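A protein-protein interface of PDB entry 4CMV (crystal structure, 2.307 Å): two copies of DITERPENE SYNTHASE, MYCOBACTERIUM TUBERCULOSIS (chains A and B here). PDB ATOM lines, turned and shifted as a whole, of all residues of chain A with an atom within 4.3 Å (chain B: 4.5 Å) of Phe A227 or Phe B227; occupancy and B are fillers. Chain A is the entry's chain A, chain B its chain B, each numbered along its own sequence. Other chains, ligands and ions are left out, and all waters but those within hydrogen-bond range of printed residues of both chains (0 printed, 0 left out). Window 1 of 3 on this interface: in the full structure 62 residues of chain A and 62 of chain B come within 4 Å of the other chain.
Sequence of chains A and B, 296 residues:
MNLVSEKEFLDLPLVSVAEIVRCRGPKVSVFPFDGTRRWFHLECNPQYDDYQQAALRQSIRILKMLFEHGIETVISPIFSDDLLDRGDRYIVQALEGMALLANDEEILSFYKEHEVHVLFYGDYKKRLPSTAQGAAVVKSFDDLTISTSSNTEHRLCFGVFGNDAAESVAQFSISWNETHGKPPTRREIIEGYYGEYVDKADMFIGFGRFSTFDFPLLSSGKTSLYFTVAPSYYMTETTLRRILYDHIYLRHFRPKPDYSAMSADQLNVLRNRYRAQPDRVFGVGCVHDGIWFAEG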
ATOM      1  N   GLY A 206     -27.116 -23.909  18.819  1.00  0.00           N
ATOM      2  CA  GLY A 206     -27.996 -23.184  17.934  1.00  0.00           C
ATOM      3  C   GLY A 206     -28.335 -24.022  16.723  1.00  0.00           C
ATOM      4  O   GLY A 206     -28.029 -25.220  16.672  1.00  0.00           O
ATOM      5  N   PHE A 207     -28.984 -23.382  15.756  1.00  0.00           N
ATOM      6  CA  PHE A 207     -29.466 -24.033  14.559  1.00  0.00           C
ATOM      7  C   PHE A 207     -29.413 -23.071  13.371  1.00  0.00           C
ATOM      8  O   PHE A 207     -29.557 -21.855  13.551  1.00  0.00           O
ATOM      9  CB  PHE A 207     -30.893 -24.534  14.774  1.00  0.00           C
ATOM     10  CG  PHE A 207     -31.698 -24.637  13.501  1.00  0.00           C
ATOM     11  CD1 PHE A 207     -31.528 -25.712  12.645  1.00  0.00           C
ATOM     12  CD2 PHE A 207     -32.598 -23.636  13.154  1.00  0.00           C
ATOM     13  CE1 PHE A 207     -32.260 -25.799  11.463  1.00  0.00           C
ATOM     14  CE2 PHE A 207     -33.318 -23.706  11.985  1.00  0.00           C
ATOM     15  CZ  PHE A 207     -33.157 -24.786  11.133  1.00  0.00           C
ATOM     16  N   GLY A 208     -29.203 -23.612  12.171  1.00  0.00           N
ATOM     17  CA  GLY A 208     -29.290 -22.831  10.943  1.00  0.00           C
ATOM     18  C   GLY A 208     -28.318 -21.658  10.894  1.00  0.00           C
ATOM     19  O   GLY A 208     -27.115 -21.829  11.114  1.00  0.00           O
ATOM     20  N   PHE A 210     -25.976 -18.815  11.779  1.00  0.00           N
ATOM     21  CA  PHE A 210     -25.137 -18.736  12.964  1.00  0.00           C
ATOM     22  C   PHE A 210     -25.560 -17.508  13.766  1.00  0.00           C
ATOM     23  O   PHE A 210     -25.310 -16.373  13.349  1.00  0.00           O
ATOM     24  CB  PHE A 210     -23.652 -18.650  12.598  1.00  0.00           C
ATOM     25  CG  PHE A 210     -23.078 -19.918  11.995  1.00  0.00           C
ATOM     26  CD1 PHE A 210     -23.897 -20.982  11.634  1.00  0.00           C
ATOM     27  CD2 PHE A 210     -21.697 -20.033  11.778  1.00  0.00           C
ATOM     28  CE1 PHE A 210     -23.350 -22.146  11.065  1.00  0.00           C
ATOM     29  CE2 PHE A 210     -21.140 -21.199  11.208  1.00  0.00           C
ATOM     30  CZ  PHE A 210     -21.972 -22.254  10.855  1.00  0.00           C
ATOM     31  N   SER A 211     -26.224 -17.749  14.894  1.00  0.00           N
ATOM     32  CA  SER A 211     -26.729 -16.690  15.766  1.00  0.00           C
ATOM     33  C   SER A 211     -26.987 -17.245  17.168  1.00  0.00           C
ATOM     34  O   SER A 211     -27.274 -18.442  17.333  1.00  0.00           O
ATOM     35  CB  SER A 211     -28.004 -16.066  15.199  1.00  0.00           C
ATOM     36  OG  SER A 211     -29.076 -16.985  15.251  1.00  0.00           O
ATOM     37  N   LEU A 225     -19.727 -22.533  21.165  1.00  0.00           N
ATOM     38  CA  LEU A 225     -20.868 -22.315  20.276  1.00  0.00           C
ATOM     39  C   LEU A 225     -21.002 -23.432  19.261  1.00  0.00           C
ATOM     40  O   LEU A 225     -20.008 -23.857  18.676  1.00  0.00           O
ATOM     41  CB  LEU A 225     -20.716 -20.980  19.543  1.00  0.00           C
ATOM     42  CG  LEU A 225     -21.251 -19.673  20.134  1.00  0.00           C
ATOM     43  CD1 LEU A 225     -21.537 -19.744  21.629  1.00  0.00           C
ATOM     44  CD2 LEU A 225     -20.370 -18.483  19.763  1.00  0.00           C
ATOM     45  N   TYR A 226     -22.227 -23.894  19.032  1.00  0.00           N
ATOM     46  CA  TYR A 226     -22.477 -24.919  18.028  1.00  0.00           C
ATOM     47  C   TYR A 226     -23.706 -24.519  17.210  1.00  0.00           C
ATOM     48  O   TYR A 226     -24.562 -23.810  17.718  1.00  0.00           O
ATOM     49  CB  TYR A 226     -22.689 -26.278  18.686  1.00  0.00           C
ATOM     50  CG  TYR A 226     -21.530 -26.689  19.554  1.00  0.00           C
ATOM     51  CD1 TYR A 226     -20.444 -27.350  19.008  1.00  0.00           C
ATOM     52  CD2 TYR A 226     -21.493 -26.367  20.907  1.00  0.00           C
ATOM     53  CE1 TYR A 226     -19.362 -27.726  19.787  1.00  0.00           C
ATOM     54  CE2 TYR A 226     -20.404 -26.747  21.706  1.00  0.00           C
ATOM     55  CZ  TYR A 226     -19.343 -27.421  21.129  1.00  0.00           C
ATOM     56  OH  TYR A 226     -18.244 -27.790  21.881  1.00  0.00           O
ATOM     57  N   PHE A 227     -23.781 -24.945  15.954  1.00  0.00           N
ATOM     58  CA  PHE A 227     -24.945 -24.672  15.127  1.00  0.00           C
ATOM     59  C   PHE A 227     -25.262 -25.902  14.324  1.00  0.00           C
ATOM     60  O   PHE A 227     -24.528 -26.245  13.379  1.00  0.00           O
ATOM     61  CB  PHE A 227     -24.705 -23.466  14.194  1.00  0.00           C
ATOM     62  CG  PHE A 227     -24.256 -22.259  14.933  1.00  0.00           C
ATOM     63  CD1 PHE A 227     -25.180 -21.481  15.605  1.00  0.00           C
ATOM     64  CD2 PHE A 227     -22.903 -21.960  15.047  1.00  0.00           C
ATOM     65  CE1 PHE A 227     -24.767 -20.391  16.379  1.00  0.00           C
ATOM     66  CE2 PHE A 227     -22.476 -20.866  15.787  1.00  0.00           C
ATOM     67  CZ  PHE A 227     -23.405 -20.079  16.452  1.00  0.00           C
ATOM     68  N   THR A 228     -26.359 -26.562  14.678  1.00  0.00           N
ATOM     69  CA  THR A 228     -26.756 -27.747  13.922  1.00  0.00           C
ATOM     70  C   THR A 228     -27.240 -27.325  12.537  1.00  0.00           C
ATOM     71  O   THR A 228     -27.631 -26.168  12.334  1.00  0.00           O
ATOM     72  CB  THR A 228     -27.860 -28.544  14.638  1.00  0.00           C
ATOM     73  OG1 THR A 228     -29.082 -27.800  14.595  1.00  0.00           O
ATOM     74  CG2 THR A 228     -27.469 -28.820  16.095  1.00  0.00           C
ATOM     75  N   VAL A 229     -27.168 -28.249  11.578  1.00  0.00           N
ATOM     76  CA  VAL A 229     -27.757 -28.037  10.262  1.00  0.00           C
ATOM     77  C   VAL A 229     -29.226 -28.404  10.329  1.00  0.00           C
ATOM     78  O   VAL A 229     -30.099 -27.679   9.850  1.00  0.00           O
ATOM     79  CB  VAL A 229     -27.086 -28.901   9.167  1.00  0.00           C
ATOM     80  CG1 VAL A 229     -27.881 -28.819   7.839  1.00  0.00           C
ATOM     81  CG2 VAL A 229     -25.647 -28.500   8.981  1.00  0.00           C
ATOM     82  N   VAL A 281     -14.822 -18.742   5.375  1.00  0.00           N
ATOM     83  CA  VAL A 281     -15.496 -18.192   6.532  1.00  0.00           C
ATOM     84  C   VAL A 281     -16.711 -19.039   6.923  1.00  0.00           C
ATOM     85  O   VAL A 281     -17.666 -19.168   6.146  1.00  0.00           O
ATOM     86  CB  VAL A 281     -15.918 -16.743   6.278  1.00  0.00           C
ATOM     87  CG1 VAL A 281     -16.578 -16.155   7.525  1.00  0.00           C
ATOM     88  CG2 VAL A 281     -14.703 -15.900   5.929  1.00  0.00           C
ATOM     89  N   PHE A 282     -16.665 -19.641   8.114  1.00  0.00           N
ATOM     90  CA  PHE A 282     -17.827 -20.369   8.596  1.00  0.00           C
ATOM     91  C   PHE A 282     -18.892 -19.359   9.011  1.00  0.00           C
ATOM     92  O   PHE A 282     -18.600 -18.367   9.704  1.00  0.00           O
ATOM     93  CB  PHE A 282     -17.456 -21.324   9.733  1.00  0.00           C
ATOM     94  CG  PHE A 282     -16.707 -22.542   9.252  1.00  0.00           C
ATOM     95  CD1 PHE A 282     -17.363 -23.520   8.520  1.00  0.00           C
ATOM     96  CD2 PHE A 282     -15.352 -22.677   9.467  1.00  0.00           C
ATOM     97  CE1 PHE A 282     -16.680 -24.636   8.030  1.00  0.00           C
ATOM     98  CE2 PHE A 282     -14.665 -23.778   8.993  1.00  0.00           C
ATOM     99  CZ  PHE A 282     -15.327 -24.768   8.273  1.00  0.00           C
ATOM    100  N   GLY B 206     -15.579 -13.617  14.147  1.00  0.00           N
ATOM    101  CA  GLY B 206     -14.700 -14.354  15.027  1.00  0.00           C
ATOM    102  C   GLY B 206     -13.690 -15.187  14.269  1.00  0.00           C
ATOM    103  O   GLY B 206     -13.545 -15.050  13.054  1.00  0.00           O
ATOM    104  N   PHE B 207     -12.970 -16.035  15.000  1.00  0.00           N
ATOM    105  CA  PHE B 207     -11.871 -16.826  14.450  1.00  0.00           C
ATOM    106  C   PHE B 207     -11.789 -18.173  15.155  1.00  0.00           C
ATOM    107  O   PHE B 207     -12.143 -18.269  16.336  1.00  0.00           O
ATOM    108  CB  PHE B 207     -10.535 -16.076  14.593  1.00  0.00           C
ATOM    109  CG  PHE B 207      -9.336 -16.987  14.671  1.00  0.00           C
ATOM    110  CD1 PHE B 207      -8.826 -17.579  13.533  1.00  0.00           C
ATOM    111  CD2 PHE B 207      -8.747 -17.277  15.889  1.00  0.00           C
ATOM    112  CE1 PHE B 207      -7.747 -18.427  13.596  1.00  0.00           C
ATOM    113  CE2 PHE B 207      -7.674 -18.135  15.965  1.00  0.00           C
ATOM    114  CZ  PHE B 207      -7.169 -18.714  14.808  1.00  0.00           C
ATOM    115  N   GLY B 208     -11.350 -19.213  14.438  1.00  0.00           N
ATOM    116  CA  GLY B 208     -11.070 -20.498  15.063  1.00  0.00           C
ATOM    117  C   GLY B 208     -12.254 -21.101  15.808  1.00  0.00           C
ATOM    118  O   GLY B 208     -13.345 -21.218  15.249  1.00  0.00           O
ATOM    119  N   PHE B 210     -15.519 -21.620  17.749  1.00  0.00           N
ATOM    120  CA  PHE B 210     -16.737 -20.823  17.649  1.00  0.00           C
ATOM    121  C   PHE B 210     -17.037 -20.221  19.011  1.00  0.00           C
ATOM    122  O   PHE B 210     -17.417 -20.929  19.949  1.00  0.00           O
ATOM    123  CB  PHE B 210     -17.927 -21.656  17.160  1.00  0.00           C
ATOM    124  CG  PHE B 210     -17.838 -22.092  15.702  1.00  0.00           C
ATOM    125  CD1 PHE B 210     -16.655 -21.955  14.982  1.00  0.00           C
ATOM    126  CD2 PHE B 210     -18.960 -22.609  15.053  1.00  0.00           C
ATOM    127  CE1 PHE B 210     -16.576 -22.354  13.660  1.00  0.00           C
ATOM    128  CE2 PHE B 210     -18.904 -22.990  13.726  1.00  0.00           C
ATOM    129  CZ  PHE B 210     -17.714 -22.865  13.024  1.00  0.00           C
ATOM    130  N   SER B 211     -16.834 -18.909  19.107  1.00  0.00           N
ATOM    131  CA  SER B 211     -16.971 -18.169  20.352  1.00  0.00           C
ATOM    132  C   SER B 211     -17.114 -16.690  20.045  1.00  0.00           C
ATOM    133  O   SER B 211     -16.530 -16.204  19.081  1.00  0.00           O
ATOM    134  CB  SER B 211     -15.751 -18.409  21.251  1.00  0.00           C
ATOM    135  OG  SER B 211     -14.590 -17.818  20.679  1.00  0.00           O
ATOM    136  N   THR B 212     -17.870 -15.981  20.877  1.00  0.00           N
ATOM    137  CA  THR B 212     -17.984 -14.528  20.801  1.00  0.00           C
ATOM    138  C   THR B 212     -17.716 -13.966  22.174  1.00  0.00           C
ATOM    139  O   THR B 212     -17.855 -14.684  23.163  1.00  0.00           O
ATOM    140  CB  THR B 212     -19.365 -14.065  20.354  1.00  0.00           C
ATOM    141  OG1 THR B 212     -20.293 -14.329  21.410  1.00  0.00           O
ATOM    142  CG2 THR B 212     -19.783 -14.792  19.065  1.00  0.00           C
ATOM    143  N   LEU B 225     -23.379 -14.086  12.926  1.00  0.00           N
ATOM    144  CA  LEU B 225     -22.114 -14.602  13.469  1.00  0.00           C
ATOM    145  C   LEU B 225     -21.267 -15.241  12.378  1.00  0.00           C
ATOM    146  O   LEU B 225     -21.805 -15.957  11.537  1.00  0.00           O
ATOM    147  CB  LEU B 225     -22.392 -15.617  14.586  1.00  0.00           C
ATOM    148  CG  LEU B 225     -22.413 -15.135  16.041  1.00  0.00           C
ATOM    149  CD1 LEU B 225     -22.809 -13.656  16.196  1.00  0.00           C
ATOM    150  CD2 LEU B 225     -23.284 -16.036  16.879  1.00  0.00           C
ATOM    151  N   TYR B 226     -19.960 -14.972  12.388  1.00  0.00           N
ATOM    152  CA  TYR B 226     -18.992 -15.538  11.430  1.00  0.00           C
ATOM    153  C   TYR B 226     -17.754 -16.011  12.168  1.00  0.00           C
ATOM    154  O   TYR B 226     -17.455 -15.517  13.256  1.00  0.00           O
ATOM    155  CB  TYR B 226     -18.589 -14.507  10.363  1.00  0.00           C
ATOM    156  CG  TYR B 226     -19.779 -14.011   9.606  1.00  0.00           C
ATOM    157  CD1 TYR B 226     -20.497 -12.924  10.061  1.00  0.00           C
ATOM    158  CD2 TYR B 226     -20.218 -14.655   8.468  1.00  0.00           C
ATOM    159  CE1 TYR B 226     -21.596 -12.488   9.413  1.00  0.00           C
ATOM    160  CE2 TYR B 226     -21.348 -14.207   7.792  1.00  0.00           C
ATOM    161  CZ  TYR B 226     -22.025 -13.125   8.282  1.00  0.00           C
ATOM    162  OH  TYR B 226     -23.161 -12.657   7.661  1.00  0.00           O
ATOM    163  N   PHE B 227     -17.057 -16.992  11.616  1.00  0.00           N
ATOM    164  CA  PHE B 227     -15.789 -17.428  12.192  1.00  0.00           C
ATOM    165  C   PHE B 227     -14.826 -17.763  11.085  1.00  0.00           C
ATOM    166  O   PHE B 227     -15.054 -18.714  10.324  1.00  0.00           O
ATOM    167  CB  PHE B 227     -15.993 -18.618  13.128  1.00  0.00           C
ATOM    168  CG  PHE B 227     -17.044 -18.373  14.139  1.00  0.00           C
ATOM    169  CD1 PHE B 227     -16.773 -17.583  15.236  1.00  0.00           C
ATOM    170  CD2 PHE B 227     -18.327 -18.899  13.979  1.00  0.00           C
ATOM    171  CE1 PHE B 227     -17.761 -17.315  16.164  1.00  0.00           C
ATOM    172  CE2 PHE B 227     -19.317 -18.643  14.900  1.00  0.00           C
ATOM    173  CZ  PHE B 227     -19.038 -17.855  15.992  1.00  0.00           C
ATOM    174  N   THR B 228     -13.785 -16.943  10.949  1.00  0.00           N
ATOM    175  CA  THR B 228     -12.779 -17.188   9.938  1.00  0.00           C
ATOM    176  C   THR B 228     -11.955 -18.382  10.367  1.00  0.00           C
ATOM    177  O   THR B 228     -11.859 -18.694  11.561  1.00  0.00           O
ATOM    178  CB  THR B 228     -11.871 -15.943   9.681  1.00  0.00           C
ATOM    179  OG1 THR B 228     -11.050 -15.679  10.825  1.00  0.00           O
ATOM    180  CG2 THR B 228     -12.723 -14.702   9.380  1.00  0.00           C
ATOM    181  N   VAL B 229     -11.381 -19.066   9.387  1.00  0.00           N
ATOM    182  CA  VAL B 229     -10.456 -20.166   9.627  1.00  0.00           C
ATOM    183  C   VAL B 229      -9.042 -19.632   9.816  1.00  0.00           C
ATOM    184  O   VAL B 229      -8.337 -20.015  10.750  1.00  0.00           O
ATOM    185  CB  VAL B 229     -10.488 -21.168   8.454  1.00  0.00           C
ATOM    186  CG1 VAL B 229      -9.437 -22.241   8.643  1.00  0.00           C
ATOM    187  CG2 VAL B 229     -11.876 -21.783   8.353  1.00  0.00           C
ATOM    188  N   VAL B 281     -22.659 -30.709  12.527  1.00  0.00           N
ATOM    189  CA  VAL B 281     -22.829 -29.733  13.577  1.00  0.00           C
ATOM    190  C   VAL B 281     -21.669 -28.788  13.374  1.00  0.00           C
ATOM    191  O   VAL B 281     -20.512 -29.197  13.482  1.00  0.00           O
ATOM    192  CB  VAL B 281     -22.791 -30.347  14.991  1.00  0.00           C
ATOM    193  CG1 VAL B 281     -22.845 -29.250  16.038  1.00  0.00           C
ATOM    194  CG2 VAL B 281     -23.917 -31.358  15.190  1.00  0.00           C
ATOM    195  N   PHE B 282     -21.954 -27.546  13.004  1.00  0.00           N
ATOM    196  CA  PHE B 282     -20.877 -26.587  12.861  1.00  0.00           C
ATOM    197  C   PHE B 282     -20.445 -26.132  14.236  1.00  0.00           C
ATOM    198  O   PHE B 282     -21.274 -25.720  15.066  1.00  0.00           O
ATOM    199  CB  PHE B 282     -21.309 -25.428  11.973  1.00  0.00           C
ATOM    200  CG  PHE B 282     -21.414 -25.808  10.521  1.00  0.00           C
ATOM    201  CD1 PHE B 282     -20.274 -26.005   9.764  1.00  0.00           C
ATOM    202  CD2 PHE B 282     -22.651 -26.028   9.931  1.00  0.00           C
ATOM    203  CE1 PHE B 282     -20.360 -26.383   8.424  1.00  0.00           C
ATOM    204  CE2 PHE B 282     -22.752 -26.408   8.613  1.00  0.00           C
ATOM    205  CZ  PHE B 282     -21.600 -26.588   7.848  1.00  0.00           C
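Of the 13 printed residues of chain B, 9 touch a printed residue of chain A.
Along chain B the printed residues that touch a printed residue of chain A span positions 210 to 282.
Of the 12 printed residues of chain A, 8 touch a printed residue of chain B.
Among the printed residues, no Asp or Glu carboxylate lies within 4 Å of a Lys or Arg side-chain nitrogen of the other chain.
Phe A210 touches Leu B225, and with the chains exchanged Leu A225 touches Phe B210.
Phe A210 touches Phe B282, and with the chains exchanged Phe A282 touches Phe B210.
Phe A227 touches Val B281, and with the chains exchanged Val A281 touches Phe B227.
Val A229 touches Phe B282, and with the chains exchanged Phe A282 touches Val B229.
The backbone NH (N) of Leu A225 lies within hydrogen-bond range of the backbone carbonyl oxygen (O) of Phe B210, at 3.1 Å.
The backbone carbonyl oxygen (O) of Phe A282 lies within hydrogen-bond range of the backbone NH (N) of Phe B227 (2.8 Å).
The backbone carbonyl oxygen of Phe A210 sits at hydrogen-bond distance from the backbone NH of Leu B225 (3.0 Å).
The backbone carbonyl oxygen of Phe B282 lies within hydrogen-bond range of the backbone NH of Phe A227, 2.8 Å away.
Of the printed residues of chain B, Phe A227 touches Phe B210 (3.99 Å), Phe B227 (3.96 Å), Val B281 (3.8 Å) and Phe B282 (2.8 Å).
Thr A228 touches none of the printed residues of chain B.
Printed residues of chain B within 4 Å of Val A281: Tyr B226 and Phe B227.
Of the printed residues of chain A, Thr B212 touches Leu A225.
Printed residues of chain A within 4 Å of Leu B225: Phe A210 (3.0 Å) and Ser A211 (3.7 Å).
Of the printed residues of chain A, Tyr B226 touches Val A281 (3.8 Å) and Phe A282 (3.3 Å).
Of chain A, only Phe A227, Val A281 and Phe A282 come within 4 Å of Phe B227.
Of the printed residues of chain A, Phe B282 touches Phe A210, Tyr A226, Phe A227 and Val A229.
The nearest printed residue of chain B that does not touch Phe A227 is Leu B225 (4.1 Å).
The nearest residue of chain A that does not touch Phe B227 is Leu A225 (4.05 Å).
The nearest printed residue of chain B that does not touch Phe A210 is Phe B227 (4.2 Å).
Among the printed residues, pairs that only touch across the chains: Tyr A226 with Phe B282, Phe A282 with Tyr B226, Phe A210 with Phe B282, Leu A225 with Ser B211, Phe A282 with Val B229, Val A229 with Phe B282, Phe A282 with Phe B210, Ser A211 with Leu B225, Leu A225 with Thr B212, Val A281 with Phe B227, Phe A210 with Phe B210, Phe A227 with Val B281, Val A281 with Tyr B226, Phe A227 with Phe B227, Tyr A226 with Val B281 and Phe A227 with Phe B210.
The backbone carbonyl oxygen of Tyr B226 lies within hydrogen-bond range of the backbone NH of Gly B206, 2.8 Å away.
O of Tyr A226 is in hydrogen-bond range of N of Gly A206 (2.8 Å).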
